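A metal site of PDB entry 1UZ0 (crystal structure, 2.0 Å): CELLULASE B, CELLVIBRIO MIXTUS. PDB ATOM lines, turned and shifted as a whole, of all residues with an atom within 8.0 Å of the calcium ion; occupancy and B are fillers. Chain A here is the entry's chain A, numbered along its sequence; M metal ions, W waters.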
ATOM      1  N   GLN A  14      25.960  10.740 -12.572  1.00  0.00           N
ATOM      2  CA  GLN A  14      24.964  10.261 -13.560  1.00  0.00           C
ATOM      3  C   GLN A  14      25.608  10.077 -14.918  1.00  0.00           C
ATOM      4  O   GLN A  14      26.730  10.555 -15.149  1.00  0.00           O
ATOM      5  CB  GLN A  14      23.858  11.250 -13.704  1.00  0.00           C
ATOM      6  CG  GLN A  14      24.326  12.593 -14.251  1.00  0.00           C
ATOM      7  CD  GLN A  14      24.185  12.713 -15.778  1.00  0.00           C
ATOM      8  OE1 GLN A  14      23.255  12.180 -16.370  1.00  0.00           O
ATOM      9  NE2 GLN A  14      25.128  13.413 -16.401  1.00  0.00           N
ATOM     10  N   SER A  15      24.919   9.405 -15.823  1.00  0.00           N
ATOM     11  CA  SER A  15      25.347   9.367 -17.194  1.00  0.00           C
ATOM     12  C   SER A  15      24.194   9.536 -18.148  1.00  0.00           C
ATOM     13  O   SER A  15      23.148   8.838 -18.056  1.00  0.00           O
ATOM     14  CB  SER A  15      26.106   8.087 -17.482  1.00  0.00           C
ATOM     15  OG  SER A  15      26.401   8.057 -18.865  1.00  0.00           O
ATOM     16  N   GLY A  16      24.323  10.559 -18.998  1.00  0.00           N
ATOM     17  CA  GLY A  16      23.447  10.780 -20.132  1.00  0.00           C
ATOM     18  C   GLY A  16      22.143  11.559 -19.974  1.00  0.00           C
ATOM     19  O   GLY A  16      21.405  11.736 -20.915  1.00  0.00           O
ATOM     20  N   THR A  17      21.865  12.068 -18.782  1.00  0.00           N
ATOM     21  CA  THR A  17      20.658  12.810 -18.515  1.00  0.00           C
ATOM     22  C   THR A  17      20.902  14.286 -18.327  1.00  0.00           C
ATOM     23  O   THR A  17      22.044  14.767 -18.339  1.00  0.00           O
ATOM     24  CB  THR A  17      19.994  12.222 -17.245  1.00  0.00           C
ATOM     25  OG1 THR A  17      20.743  12.618 -16.082  1.00  0.00           O
ATOM     26  CG2 THR A  17      19.968  10.690 -17.322  1.00  0.00           C
ATOM     27  N   GLN A  18      19.820  15.019 -18.178  1.00  0.00           N
ATOM     28  CA  GLN A  18      19.889  16.404 -17.884  1.00  0.00           C
ATOM     29  C   GLN A  18      18.741  16.793 -17.005  1.00  0.00           C
ATOM     30  O   GLN A  18      17.658  16.233 -17.091  1.00  0.00           O
ATOM     31  CB  GLN A  18      19.897  17.209 -19.198  1.00  0.00           C
ATOM     32  CG  GLN A  18      20.152  18.696 -19.001  1.00  0.00           C
ATOM     33  CD  GLN A  18      21.490  19.069 -18.261  1.00  0.00           C
ATOM     34  OE1 GLN A  18      21.476  19.502 -17.064  1.00  0.00           O
ATOM     35  NE2 GLN A  18      22.623  18.960 -18.990  1.00  0.00           N
ATOM     36  N   GLY A  32      15.374  14.656 -16.786  1.00  0.00           N
ATOM     37  CA  GLY A  32      14.817  14.291 -18.087  1.00  0.00           C
ATOM     38  C   GLY A  32      15.876  13.759 -19.043  1.00  0.00           C
ATOM     39  O   GLY A  32      17.044  13.534 -18.645  1.00  0.00           O
ATOM     40  N   TYR A  33      15.508  13.708 -20.324  1.00  0.00           N
ATOM     41  CA  TYR A  33      16.369  13.261 -21.385  1.00  0.00           C
ATOM     42  C   TYR A  33      16.962  11.915 -21.055  1.00  0.00           C
ATOM     43  O   TYR A  33      18.162  11.694 -21.236  1.00  0.00           O
ATOM     44  CB  TYR A  33      17.494  14.318 -21.675  1.00  0.00           C
ATOM     45  CG  TYR A  33      16.922  15.625 -22.008  1.00  0.00           C
ATOM     46  CD1 TYR A  33      16.511  16.489 -21.005  1.00  0.00           C
ATOM     47  CD2 TYR A  33      16.732  16.026 -23.340  1.00  0.00           C
ATOM     48  CE1 TYR A  33      15.956  17.676 -21.298  1.00  0.00           C
ATOM     49  CE2 TYR A  33      16.168  17.243 -23.633  1.00  0.00           C
ATOM     50  CZ  TYR A  33      15.760  18.058 -22.609  1.00  0.00           C
ATOM     51  OH  TYR A  33      15.178  19.286 -22.808  1.00  0.00           O
ATOM     52  N   ILE A  34      16.114  11.005 -20.573  1.00  0.00           N
ATOM     53  CA  ILE A  34      16.533   9.677 -20.178  1.00  0.00           C
ATOM     54  C   ILE A  34      16.348   8.720 -21.341  1.00  0.00           C
ATOM     55  O   ILE A  34      15.256   8.585 -21.885  1.00  0.00           O
ATOM     56  CB  ILE A  34      15.755   9.197 -18.914  1.00  0.00           C
ATOM     57  CG1 ILE A  34      15.868  10.203 -17.752  1.00  0.00           C
ATOM     58  CG2 ILE A  34      16.198   7.810 -18.431  1.00  0.00           C
ATOM     59  CD1 ILE A  34      15.038   9.772 -16.501  1.00  0.00           C
ATOM     60  N   ASP A  35      17.438   8.075 -21.714  1.00  0.00           N
ATOM     61  CA  ASP A  35      17.508   7.045 -22.719  1.00  0.00           C
ATOM     62  C   ASP A  35      18.019   5.710 -22.175  1.00  0.00           C
ATOM     63  O   ASP A  35      18.680   5.614 -21.123  1.00  0.00           O
ATOM     64  CB  ASP A  35      18.385   7.508 -23.855  1.00  0.00           C
ATOM     65  CG  ASP A  35      17.991   8.866 -24.354  1.00  0.00           C
ATOM     66  OD1 ASP A  35      16.877   8.999 -24.950  1.00  0.00           O
ATOM     67  OD2 ASP A  35      18.676   9.880 -24.169  1.00  0.00           O
ATOM     68  N   ALA A  36      17.665   4.646 -22.889  1.00  0.00           N
ATOM     69  CA  ALA A  36      18.180   3.308 -22.608  1.00  0.00           C
ATOM     70  C   ALA A  36      19.681   3.347 -22.330  1.00  0.00           C
ATOM     71  O   ALA A  36      20.431   3.942 -23.118  1.00  0.00           O
ATOM     72  CB  ALA A  36      17.913   2.369 -23.780  1.00  0.00           C
ATOM     73  N   GLY A  37      20.078   2.747 -21.205  1.00  0.00           N
ATOM     74  CA  GLY A  37      21.467   2.767 -20.720  1.00  0.00           C
ATOM     75  C   GLY A  37      21.898   3.934 -19.866  1.00  0.00           C
ATOM     76  O   GLY A  37      22.928   3.890 -19.210  1.00  0.00           O
ATOM     77  N   ASP A  38      21.143   5.021 -19.869  1.00  0.00           N
ATOM     78  CA  ASP A  38      21.416   6.127 -18.932  1.00  0.00           C
ATOM     79  C   ASP A  38      21.218   5.679 -17.485  1.00  0.00           C
ATOM     80  O   ASP A  38      20.498   4.710 -17.181  1.00  0.00           O
ATOM     81  CB  ASP A  38      20.561   7.359 -19.205  1.00  0.00           C
ATOM     82  CG  ASP A  38      20.838   7.989 -20.564  1.00  0.00           C
ATOM     83  OD1 ASP A  38      21.910   7.761 -21.162  1.00  0.00           O
ATOM     84  OD2 ASP A  38      20.037   8.779 -21.080  1.00  0.00           O
ATOM     85  N   TRP A  39      21.828   6.411 -16.559  1.00  0.00           N
ATOM     86  CA  TRP A  39      21.796   6.016 -15.147  1.00  0.00           C
ATOM     87  C   TRP A  39      22.055   7.161 -14.229  1.00  0.00           C
ATOM     88  O   TRP A  39      22.586   8.207 -14.578  1.00  0.00           O
ATOM     89  CB  TRP A  39      22.741   4.826 -14.876  1.00  0.00           C
ATOM     90  CG  TRP A  39      24.224   5.048 -15.224  1.00  0.00           C
ATOM     91  CD1 TRP A  39      24.897   4.608 -16.330  1.00  0.00           C
ATOM     92  CD2 TRP A  39      25.197   5.764 -14.449  1.00  0.00           C
ATOM     93  NE1 TRP A  39      26.220   4.982 -16.284  1.00  0.00           N
ATOM     94  CE2 TRP A  39      26.439   5.689 -15.123  1.00  0.00           C
ATOM     95  CE3 TRP A  39      25.152   6.437 -13.230  1.00  0.00           C
ATOM     96  CZ2 TRP A  39      27.602   6.305 -14.665  1.00  0.00           C
ATOM     97  CZ3 TRP A  39      26.317   7.043 -12.763  1.00  0.00           C
ATOM     98  CH2 TRP A  39      27.530   6.967 -13.493  1.00  0.00           C
ATOM     99  N   ALA A 115      18.053   3.203 -16.563  1.00  0.00           N
ATOM    100  CA  ALA A 115      17.046   3.204 -17.575  1.00  0.00           C
ATOM    101  C   ALA A 115      17.233   2.026 -18.554  1.00  0.00           C
ATOM    102  O   ALA A 115      18.233   1.945 -19.296  1.00  0.00           O
ATOM    103  CB  ALA A 115      17.034   4.546 -18.309  1.00  0.00           C
ATOM    104  N   GLY A 118      13.971   4.344 -22.550  1.00  0.00           N
ATOM    105  CA  GLY A 118      13.826   5.754 -22.337  1.00  0.00           C
ATOM    106  C   GLY A 118      12.416   6.248 -22.403  1.00  0.00           C
ATOM    107  O   GLY A 118      11.510   5.432 -22.408  1.00  0.00           O
HETATM  108 CA    CA M   1      19.999  10.704 -22.383  1.00  0.00          CA
HETATM  109  O   HOH W   1      21.888   9.456 -23.403  1.00  0.00           O
HETATM  110  O   HOH W   2      20.510  12.677 -23.864  1.00  0.00           O
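O of Gly 16 is bound to the calcium ion, at 2.3 Å.
The side-chain carboxylate (OD2) of Asp 38 is bound to the calcium ion (2.3 Å).
OD2 of Asp 35 binds the calcium ion, at 2.4 Å.
O of Tyr 33 is bound to the calcium ion (2.4 Å).
The calcium ion is bound by water W1.
Water W2 is bound to the calcium ion (2.5 Å).
The calcium ion has six donor atoms within binding distance.
OE1 of Gln 14 sits at hydrogen-bond distance from N of Gly 16 (3.3 Å).
The backbone NH of Ala 115 is in hydrogen-bond range of the backbone carbonyl oxygen of Asp 38 (2.9 Å).
Four residues have an atom within 4 Å of the calcium ion: Gly 16, Tyr 33, Asp 35 and Asp 38.
The nearest printed residue that does not touch the calcium ion is Ile 34 (4.2 Å).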
